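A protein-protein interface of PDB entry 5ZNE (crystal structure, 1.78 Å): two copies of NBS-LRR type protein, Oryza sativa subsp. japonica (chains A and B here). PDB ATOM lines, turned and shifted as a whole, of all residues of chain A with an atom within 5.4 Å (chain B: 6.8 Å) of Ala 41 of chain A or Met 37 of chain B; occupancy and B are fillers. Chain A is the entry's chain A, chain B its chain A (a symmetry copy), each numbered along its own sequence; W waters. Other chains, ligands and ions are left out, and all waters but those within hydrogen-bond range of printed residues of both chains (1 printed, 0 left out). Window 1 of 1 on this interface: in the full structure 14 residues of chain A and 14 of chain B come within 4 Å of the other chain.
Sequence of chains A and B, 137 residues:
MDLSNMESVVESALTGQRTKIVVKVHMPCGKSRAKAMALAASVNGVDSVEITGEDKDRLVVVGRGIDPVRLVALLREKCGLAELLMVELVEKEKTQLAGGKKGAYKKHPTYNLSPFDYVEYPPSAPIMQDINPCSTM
Water W1 lies within hydrogen-bond range of the side-chain carboxylate (OD1) of Asp 47 of chain A, the backbone carbonyl oxygen (O) of Val 46 of chain A and the guanidinium group (NE) of Arg 33 of chain B.
Of the printed residues of chain B, Ala 41 of chain A touches Ala 34, Met 37 and Ala 38. Of the printed residues of chain A, Met 37 of chain B touches Ala 41 (3.7 Å), Val 46 (3.995 Å), Asp 47 (3.9 Å) and Ser 48 (3.9 Å). Of the printed residues of chain B, Asp 47 of chain A touches Met 37, Glu 50 and Ile 51. Of the printed residues of chain B, Ser 42 of chain A touches Ala 34. Printed residues of chain B within 4 Å of Ala 38 of chain A: Ala 38 and Ala 41. Ser 32 of chain B touches none of the printed residues of chain A. Arg 33 of chain B touches none of the printed residues of chain A. The nearest printed residue of chain A that does not touch Ile 51 of chain B is Ser 48 of chain A (5.1 Å).
Met 37 of chain A touches Ala 41 of chain B, and with the chains exchanged Ala 41 of chain A touches Met 37 of chain B. Ala 38 of chain A touches its own counterpart, Ala 38 of chain B. Ala 38 of chain A touches Ala 41 of chain B, and with the chains exchanged Ala 41 of chain A touches Ala 38 of chain B. Val 49 of chain B touches its own counterpart, Val 49 of chain A. Of the 14 pairs that touch across the chains among the printed residues, 6 have their exchanged pair printed and touching as well.
O of Leu 39 of chain A is in hydrogen-bond range of OG of Ser 42 of chain A (2.7 Å). The backbone NH of Val 60 of chain B lies within hydrogen-bond range of the backbone carbonyl oxygen of Glu 50 of chain B (2.7 Å).
The backbone carbonyl oxygen of Asp 47 of chain A is in hydrogen-bond range of the backbone NH of Ile 51 of chain B (2.9 Å). N of Val 49 of chain A sits at hydrogen-bond distance from O of Val 49 of chain B (2.9 Å).
Among the printed residues, merely in contact across the chains: Met 37 of chain A with Ala 41 of chain B, Ala 38 of chain A with Ala 38 of chain B, Ala 38 of chain A with Ala 41 of chain B, Ala 41 of chain A with Ala 34 of chain B, Ala 41 of chain A with Met 37 of chain B, Ala 41 of chain A with Ala 38 of chain B, Ser 42 of chain A with Ala 34 of chain B, Val 46 of chain A with Met 37 of chain B, Asp 47 of chain A with Met 37 of chain B, Asp 47 of chain A with Glu 50 of chain B, Ser 48 of chain A with Met 37 of chain B and Ser 48 of chain A with Val 49 of chain B.
Printed residues of chain B that touch a printed residue of chain A: Ala 34, Met 37, Ala 38, Ala 41, Val 49, Glu 50 and Ile 51. Hydrophobic or aromatic side chains of chain B that line the printed part of chain A: Ala 34, Met 37, Ala 38 and Ala 41. Along chain B the printed residues that touch a printed residue of chain A span positions 34 to 51. Of the 12 printed residues of chain A, 8 touch a printed residue of chain B. Hydrophobic or aromatic side chains of chain A that line the printed part of chain B: Met 37, Ala 38, Ala 41 and Val 46. Along chain A the printed residues that touch a printed residue of chain B span positions 37 to 49. Among the printed residues, no Asp or Glu carboxylate lies within 4 Å of a Lys or Arg side-chain nitrogen of the other chain.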
ATOM      1  N   ALA A  36      30.435   0.443   7.467  1.00  0.00           N
ATOM      2  CA  ALA A  36      31.401   1.357   6.877  1.00  0.00           C
ATOM      3  C   ALA A  36      30.937   2.800   6.979  1.00  0.00           C
ATOM      4  O   ALA A  36      31.755   3.703   7.199  1.00  0.00           O
ATOM      5  CB  ALA A  36      31.626   1.012   5.424  1.00  0.00           C
ATOM      6  N   MET A  37      29.648   3.037   6.711  1.00  0.00           N
ATOM      7  CA  MET A  37      29.090   4.382   6.813  1.00  0.00           C
ATOM      8  C   MET A  37      29.253   4.925   8.222  1.00  0.00           C
ATOM      9  O   MET A  37      29.635   6.084   8.416  1.00  0.00           O
ATOM     10  CB  MET A  37      27.602   4.380   6.453  1.00  0.00           C
ATOM     11  CG  MET A  37      27.259   4.234   4.988  1.00  0.00           C
ATOM     12  SD  MET A  37      26.871   5.814   4.220  1.00  0.00           S
ATOM     13  CE  MET A  37      25.440   6.308   5.169  1.00  0.00           C
ATOM     14  N   ALA A  38      28.939   4.100   9.217  1.00  0.00           N
ATOM     15  CA  ALA A  38      28.993   4.549  10.607  1.00  0.00           C
ATOM     16  C   ALA A  38      30.425   4.790  11.057  1.00  0.00           C
ATOM     17  O   ALA A  38      30.675   5.645  11.915  1.00  0.00           O
ATOM     18  CB  ALA A  38      28.330   3.514  11.511  1.00  0.00           C
ATOM     19  N   LEU A  39      31.369   4.036  10.503  1.00  0.00           N
ATOM     20  CA  LEU A  39      32.776   4.262  10.803  1.00  0.00           C
ATOM     21  C   LEU A  39      33.232   5.612  10.269  1.00  0.00           C
ATOM     22  O   LEU A  39      33.883   6.383  10.983  1.00  0.00           O
ATOM     23  CB  LEU A  39      33.618   3.131  10.215  1.00  0.00           C
ATOM     24  CG  LEU A  39      35.038   2.989  10.762  1.00  0.00           C
ATOM     25  CD1 LEU A  39      34.985   2.619  12.236  1.00  0.00           C
ATOM     26  CD2 LEU A  39      35.813   1.950   9.973  1.00  0.00           C
ATOM     27  N   ALA A  40      32.888   5.918   9.014  1.00  0.00           N
ATOM     28  CA  ALA A  40      33.255   7.211   8.441  1.00  0.00           C
ATOM     29  C   ALA A  40      32.554   8.349   9.170  1.00  0.00           C
ATOM     30  O   ALA A  40      33.163   9.396   9.430  1.00  0.00           O
ATOM     31  CB  ALA A  40      32.918   7.251   6.955  1.00  0.00           C
ATOM     32  N   ALA A  41      31.272   8.159   9.507  1.00  0.00           N
ATOM     33  CA  ALA A  41      30.500   9.205  10.178  1.00  0.00           C
ATOM     34  C   ALA A  41      31.055   9.540  11.551  1.00  0.00           C
ATOM     35  O   ALA A  41      30.843  10.658  12.047  1.00  0.00           O
ATOM     36  CB  ALA A  41      29.033   8.788  10.312  1.00  0.00           C
ATOM     37  N   SER A  42      31.734   8.588  12.195  1.00  0.00           N
ATOM     38  CA  SER A  42      32.234   8.784  13.548  1.00  0.00           C
ATOM     39  C   SER A  42      33.522   9.597  13.603  1.00  0.00           C
ATOM     40  O   SER A  42      33.934   9.990  14.700  1.00  0.00           O
ATOM     41  CB  SER A  42      32.457   7.428  14.223  1.00  0.00           C
ATOM     42  OG  SER A  42      33.540   6.750  13.615  1.00  0.00           O
ATOM     43  N   VAL A  43      34.166   9.853  12.464  1.00  0.00           N
ATOM     44  CA  VAL A  43      35.377  10.662  12.453  1.00  0.00           C
ATOM     45  C   VAL A  43      35.013  12.126  12.676  1.00  0.00           C
ATOM     46  O   VAL A  43      34.158  12.688  11.982  1.00  0.00           O
ATOM     47  CB  VAL A  43      36.141  10.457  11.135  1.00  0.00           C
ATOM     48  CG1 VAL A  43      37.375  11.341  11.080  1.00  0.00           C
ATOM     49  CG2 VAL A  43      36.526   8.988  10.972  1.00  0.00           C
ATOM     50  N   VAL A  46      33.465  15.155  10.045  1.00  0.00           N
ATOM     51  CA  VAL A  46      32.691  14.667   8.909  1.00  0.00           C
ATOM     52  C   VAL A  46      31.308  15.305   8.950  1.00  0.00           C
ATOM     53  O   VAL A  46      30.646  15.324   9.999  1.00  0.00           O
ATOM     54  CB  VAL A  46      32.612  13.130   8.935  1.00  0.00           C
ATOM     55  CG1 VAL A  46      31.647  12.619   7.878  1.00  0.00           C
ATOM     56  CG2 VAL A  46      34.005  12.492   8.728  1.00  0.00           C
ATOM     57  N   ASP A  47      30.879  15.886   7.828  1.00  0.00           N
ATOM     58  CA  ASP A  47      29.563  16.494   7.674  1.00  0.00           C
ATOM     59  C   ASP A  47      28.603  15.665   6.840  1.00  0.00           C
ATOM     60  O   ASP A  47      27.391  15.914   6.880  1.00  0.00           O
ATOM     61  CB  ASP A  47      29.677  17.874   7.005  1.00  0.00           C
ATOM     62  CG  ASP A  47      30.394  18.892   7.866  1.00  0.00           C
ATOM     63  OD1 ASP A  47      30.221  18.855   9.099  1.00  0.00           O
ATOM     64  OD2 ASP A  47      31.124  19.742   7.314  1.00  0.00           O
ATOM     65  N   SER A  48      29.119  14.736   6.042  1.00  0.00           N
ATOM     66  CA  SER A  48      28.308  14.011   5.078  1.00  0.00           C
ATOM     67  C   SER A  48      28.969  12.673   4.784  1.00  0.00           C
ATOM     68  O   SER A  48      30.193  12.608   4.611  1.00  0.00           O
ATOM     69  CB  SER A  48      28.154  14.840   3.793  1.00  0.00           C
ATOM     70  OG  SER A  48      27.500  14.122   2.772  1.00  0.00           O
ATOM     71  N   VAL A  49      28.170  11.605   4.763  1.00  0.00           N
ATOM     72  CA  VAL A  49      28.632  10.303   4.286  1.00  0.00           C
ATOM     73  C   VAL A  49      27.554   9.731   3.372  1.00  0.00           C
ATOM     74  O   VAL A  49      26.361   9.832   3.667  1.00  0.00           O
ATOM     75  CB  VAL A  49      28.953   9.318   5.438  1.00  0.00           C
ATOM     76  CG1 VAL A  49      29.436   8.018   4.890  1.00  0.00           C
ATOM     77  CG2 VAL A  49      30.009   9.875   6.378  1.00  0.00           C
ATOM     78  N   MET B  27      22.995  18.533  19.268  1.00  0.00           N
ATOM     79  CA  MET B  27      24.332  18.101  18.870  1.00  0.00           C
ATOM     80  C   MET B  27      25.309  19.265  18.895  1.00  0.00           C
ATOM     81  O   MET B  27      25.857  19.623  17.843  1.00  0.00           O
ATOM     82  CB  MET B  27      24.366  17.542  17.450  1.00  0.00           C
ATOM     83  CG  MET B  27      23.301  16.600  17.074  1.00  0.00           C
ATOM     84  SD  MET B  27      23.546  16.129  15.357  1.00  0.00           S
ATOM     85  CE  MET B  27      22.562  17.306  14.425  1.00  0.00           C
ATOM     86  N   GLY B  30      31.390  18.812  17.813  1.00  0.00           N
ATOM     87  CA  GLY B  30      31.751  17.874  16.759  1.00  0.00           C
ATOM     88  C   GLY B  30      31.617  16.428  17.195  1.00  0.00           C
ATOM     89  O   GLY B  30      31.183  15.571  16.416  1.00  0.00           O
ATOM     90  N   SER B  32      29.487  15.211  19.407  1.00  0.00           N
ATOM     91  CA  SER B  32      28.078  14.823  19.476  1.00  0.00           C
ATOM     92  C   SER B  32      27.444  14.776  18.088  1.00  0.00           C
ATOM     93  O   SER B  32      26.511  13.993  17.854  1.00  0.00           O
ATOM     94  CB  SER B  32      27.314  15.753  20.435  1.00  0.00           C
ATOM     95  OG  SER B  32      27.247  17.093  19.975  1.00  0.00           O
ATOM     96  N   ARG B  33      27.958  15.564  17.144  1.00  0.00           N
ATOM     97  CA  ARG B  33      27.510  15.433  15.763  1.00  0.00           C
ATOM     98  C   ARG B  33      27.928  14.087  15.186  1.00  0.00           C
ATOM     99  O   ARG B  33      27.162  13.448  14.453  1.00  0.00           O
ATOM    100  CB  ARG B  33      28.071  16.586  14.925  1.00  0.00           C
ATOM    101  CG  ARG B  33      27.297  17.900  15.138  1.00  0.00           C
ATOM    102  CD  ARG B  33      27.618  18.944  14.071  1.00  0.00           C
ATOM    103  NE  ARG B  33      29.026  19.341  14.083  1.00  0.00           N
ATOM    104  CZ  ARG B  33      29.520  20.370  14.764  1.00  0.00           C
ATOM    105  NH1 ARG B  33      28.729  21.137  15.512  1.00  0.00           N
ATOM    106  NH2 ARG B  33      30.819  20.636  14.696  1.00  0.00           N
ATOM    107  N   ALA B  34      29.142  13.647  15.511  1.00  0.00           N
ATOM    108  CA  ALA B  34      29.642  12.375  15.009  1.00  0.00           C
ATOM    109  C   ALA B  34      28.865  11.208  15.603  1.00  0.00           C
ATOM    110  O   ALA B  34      28.563  10.237  14.903  1.00  0.00           O
ATOM    111  CB  ALA B  34      31.137  12.252  15.313  1.00  0.00           C
ATOM    112  N   LYS B  35      28.508  11.297  16.885  1.00  0.00           N
ATOM    113  CA  LYS B  35      27.720  10.239  17.511  1.00  0.00           C
ATOM    114  C   LYS B  35      26.352  10.102  16.853  1.00  0.00           C
ATOM    115  O   LYS B  35      25.880   8.987  16.598  1.00  0.00           O
ATOM    116  CB  LYS B  35      27.570  10.514  19.010  1.00  0.00           C
ATOM    117  CG  LYS B  35      26.595   9.584  19.710  1.00  0.00           C
ATOM    118  CD  LYS B  35      26.495   9.869  21.208  1.00  0.00           C
ATOM    119  CE  LYS B  35      26.562  11.360  21.520  1.00  0.00           C
ATOM    120  NZ  LYS B  35      26.135  11.653  22.920  1.00  0.00           N
ATOM    121  N   ALA B  36      25.704  11.226  16.558  1.00  0.00           N
ATOM    122  CA  ALA B  36      24.386  11.172  15.943  1.00  0.00           C
ATOM    123  C   ALA B  36      24.460  10.684  14.507  1.00  0.00           C
ATOM    124  O   ALA B  36      23.573   9.947  14.054  1.00  0.00           O
ATOM    125  CB  ALA B  36      23.743  12.538  15.968  1.00  0.00           C
ATOM    126  N   MET B  37      25.451  11.175  13.755  1.00  0.00           N
ATOM    127  CA  MET B  37      25.634  10.745  12.373  1.00  0.00           C
ATOM    128  C   MET B  37      25.862   9.246  12.302  1.00  0.00           C
ATOM    129  O   MET B  37      25.289   8.556  11.453  1.00  0.00           O
ATOM    130  CB  MET B  37      26.831  11.459  11.738  1.00  0.00           C
ATOM    131  CG  MET B  37      26.639  12.913  11.373  1.00  0.00           C
ATOM    132  SD  MET B  37      26.291  13.134   9.622  1.00  0.00           S
ATOM    133  CE  MET B  37      27.786  12.480   8.895  1.00  0.00           C
ATOM    134  N   ALA B  38      26.723   8.734  13.177  1.00  0.00           N
ATOM    135  CA  ALA B  38      27.066   7.313  13.147  1.00  0.00           C
ATOM    136  C   ALA B  38      25.889   6.449  13.569  1.00  0.00           C
ATOM    137  O   ALA B  38      25.757   5.307  13.112  1.00  0.00           O
ATOM    138  CB  ALA B  38      28.260   7.050  14.059  1.00  0.00           C
ATOM    139  N   LEU B  39      25.041   6.969  14.450  1.00  0.00           N
ATOM    140  CA  LEU B  39      23.835   6.251  14.838  1.00  0.00           C
ATOM    141  C   LEU B  39      22.879   6.124  13.661  1.00  0.00           C
ATOM    142  O   LEU B  39      22.358   5.036  13.390  1.00  0.00           O
ATOM    143  CB  LEU B  39      23.164   6.964  16.011  1.00  0.00           C
ATOM    144  CG  LEU B  39      22.134   6.154  16.796  1.00  0.00           C
ATOM    145  CD1 LEU B  39      22.818   4.981  17.481  1.00  0.00           C
ATOM    146  CD2 LEU B  39      21.424   7.031  17.811  1.00  0.00           C
ATOM    147  N   ALA B  40      22.646   7.228  12.944  1.00  0.00           N
ATOM    148  CA  ALA B  40      21.770   7.179  11.776  1.00  0.00           C
ATOM    149  C   ALA B  40      22.366   6.300  10.684  1.00  0.00           C
ATOM    150  O   ALA B  40      21.643   5.532  10.035  1.00  0.00           O
ATOM    151  CB  ALA B  40      21.517   8.584  11.241  1.00  0.00           C
ATOM    152  N   ALA B  41      23.683   6.403  10.471  1.00  0.00           N
ATOM    153  CA  ALA B  41      24.345   5.628   9.420  1.00  0.00           C
ATOM    154  C   ALA B  41      24.264   4.132   9.670  1.00  0.00           C
ATOM    155  O   ALA B  41      24.343   3.341   8.717  1.00  0.00           O
ATOM    156  CB  ALA B  41      25.813   6.042   9.290  1.00  0.00           C
ATOM    157  N   SER B  42      24.143   3.721  10.934  1.00  0.00           N
ATOM    158  CA  SER B  42      24.141   2.307  11.284  1.00  0.00           C
ATOM    159  C   SER B  42      22.799   1.628  11.042  1.00  0.00           C
ATOM    160  O   SER B  42      22.729   0.397  11.119  1.00  0.00           O
ATOM    161  CB  SER B  42      24.544   2.133  12.751  1.00  0.00           C
ATOM    162  OG  SER B  42      23.532   2.638  13.601  1.00  0.00           O
ATOM    163  N   VAL B  49      23.814  10.223   5.049  1.00  0.00           N
ATOM    164  CA  VAL B  49      23.568  10.998   6.263  1.00  0.00           C
ATOM    165  C   VAL B  49      24.345  12.304   6.150  1.00  0.00           C
ATOM    166  O   VAL B  49      25.492  12.317   5.697  1.00  0.00           O
ATOM    167  CB  VAL B  49      23.961  10.236   7.554  1.00  0.00           C
ATOM    168  CG1 VAL B  49      23.669  11.069   8.757  1.00  0.00           C
ATOM    169  CG2 VAL B  49      23.215   8.918   7.680  1.00  0.00           C
ATOM    170  N   GLU B  50      23.720  13.405   6.568  1.00  0.00           N
ATOM    171  CA  GLU B  50      24.303  14.728   6.405  1.00  0.00           C
ATOM    172  C   GLU B  50      23.849  15.631   7.541  1.00  0.00           C
ATOM    173  O   GLU B  50      22.708  15.532   8.002  1.00  0.00           O
ATOM    174  CB  GLU B  50      23.894  15.327   5.055  1.00  0.00           C
ATOM    175  CG  GLU B  50      24.430  16.710   4.783  1.00  0.00           C
ATOM    176  CD  GLU B  50      23.953  17.256   3.451  1.00  0.00           C
ATOM    177  OE1 GLU B  50      22.816  16.928   3.049  1.00  0.00           O
ATOM    178  OE2 GLU B  50      24.712  18.010   2.808  1.00  0.00           O
ATOM    179  N   ILE B  51      24.742  16.515   7.982  1.00  0.00           N
ATOM    180  CA  ILE B  51      24.408  17.542   8.962  1.00  0.00           C
ATOM    181  C   ILE B  51      24.311  18.869   8.232  1.00  0.00           C
ATOM    182  O   ILE B  51      25.220  19.238   7.476  1.00  0.00           O
ATOM    183  CB  ILE B  51      25.434  17.592  10.104  1.00  0.00           C
ATOM    184  CG1 ILE B  51      25.297  16.301  10.907  1.00  0.00           C
ATOM    185  CG2 ILE B  51      25.157  18.816  11.023  1.00  0.00           C
ATOM    186  CD1 ILE B  51      25.944  16.313  12.224  1.00  0.00           C
ATOM    187  N   LEU B  59      19.819  16.761  11.091  1.00  0.00           N
ATOM    188  CA  LEU B  59      20.352  15.508  10.576  1.00  0.00           C
ATOM    189  C   LEU B  59      19.468  15.059   9.418  1.00  0.00           C
ATOM    190  O   LEU B  59      18.256  14.914   9.591  1.00  0.00           O
ATOM    191  CB  LEU B  59      20.371  14.470  11.695  1.00  0.00           C
ATOM    192  CG  LEU B  59      21.075  13.153  11.424  1.00  0.00           C
ATOM    193  CD1 LEU B  59      22.568  13.383  11.273  1.00  0.00           C
ATOM    194  CD2 LEU B  59      20.794  12.220  12.579  1.00  0.00           C
ATOM    195  N   VAL B  60      20.060  14.876   8.235  1.00  0.00           N
ATOM    196  CA  VAL B  60      19.316  14.507   7.034  1.00  0.00           C
ATOM    197  C   VAL B  60      19.711  13.089   6.671  1.00  0.00           C
ATOM    198  O   VAL B  60      20.901  12.805   6.471  1.00  0.00           O
ATOM    199  CB  VAL B  60      19.589  15.467   5.866  1.00  0.00           C
ATOM    200  CG1 VAL B  60      18.737  15.079   4.652  1.00  0.00           C
ATOM    201  CG2 VAL B  60      19.322  16.899   6.278  1.00  0.00           C
ATOM    202  N   LEU B  75      17.758   8.431  18.300  1.00  0.00           N
ATOM    203  CA  LEU B  75      18.495   9.684  18.442  1.00  0.00           C
ATOM    204  C   LEU B  75      18.137  10.396  19.738  1.00  0.00           C
ATOM    205  O   LEU B  75      19.013  10.962  20.401  1.00  0.00           O
ATOM    206  CB  LEU B  75      18.225  10.594  17.246  1.00  0.00           C
ATOM    207  CG  LEU B  75      18.887  10.159  15.938  1.00  0.00           C
ATOM    208  CD1 LEU B  75      18.195  10.858  14.768  1.00  0.00           C
ATOM    209  CD2 LEU B  75      20.391  10.444  15.959  1.00  0.00           C
ATOM    210  N   CYS B  79      21.262  11.070  22.069  1.00  0.00           N
ATOM    211  CA  CYS B  79      21.666  12.471  22.068  1.00  0.00           C
ATOM    212  C   CYS B  79      20.884  13.345  23.036  1.00  0.00           C
ATOM    213  O   CYS B  79      21.247  14.513  23.212  1.00  0.00           O
ATOM    214  CB  CYS B  79      21.534  13.063  20.657  1.00  0.00           C
ATOM    215  SG  CYS B  79      22.431  12.128  19.414  1.00  0.00           S
HETATM  216  O   HOH W   1      29.421  17.798  11.150  1.00  0.00           O
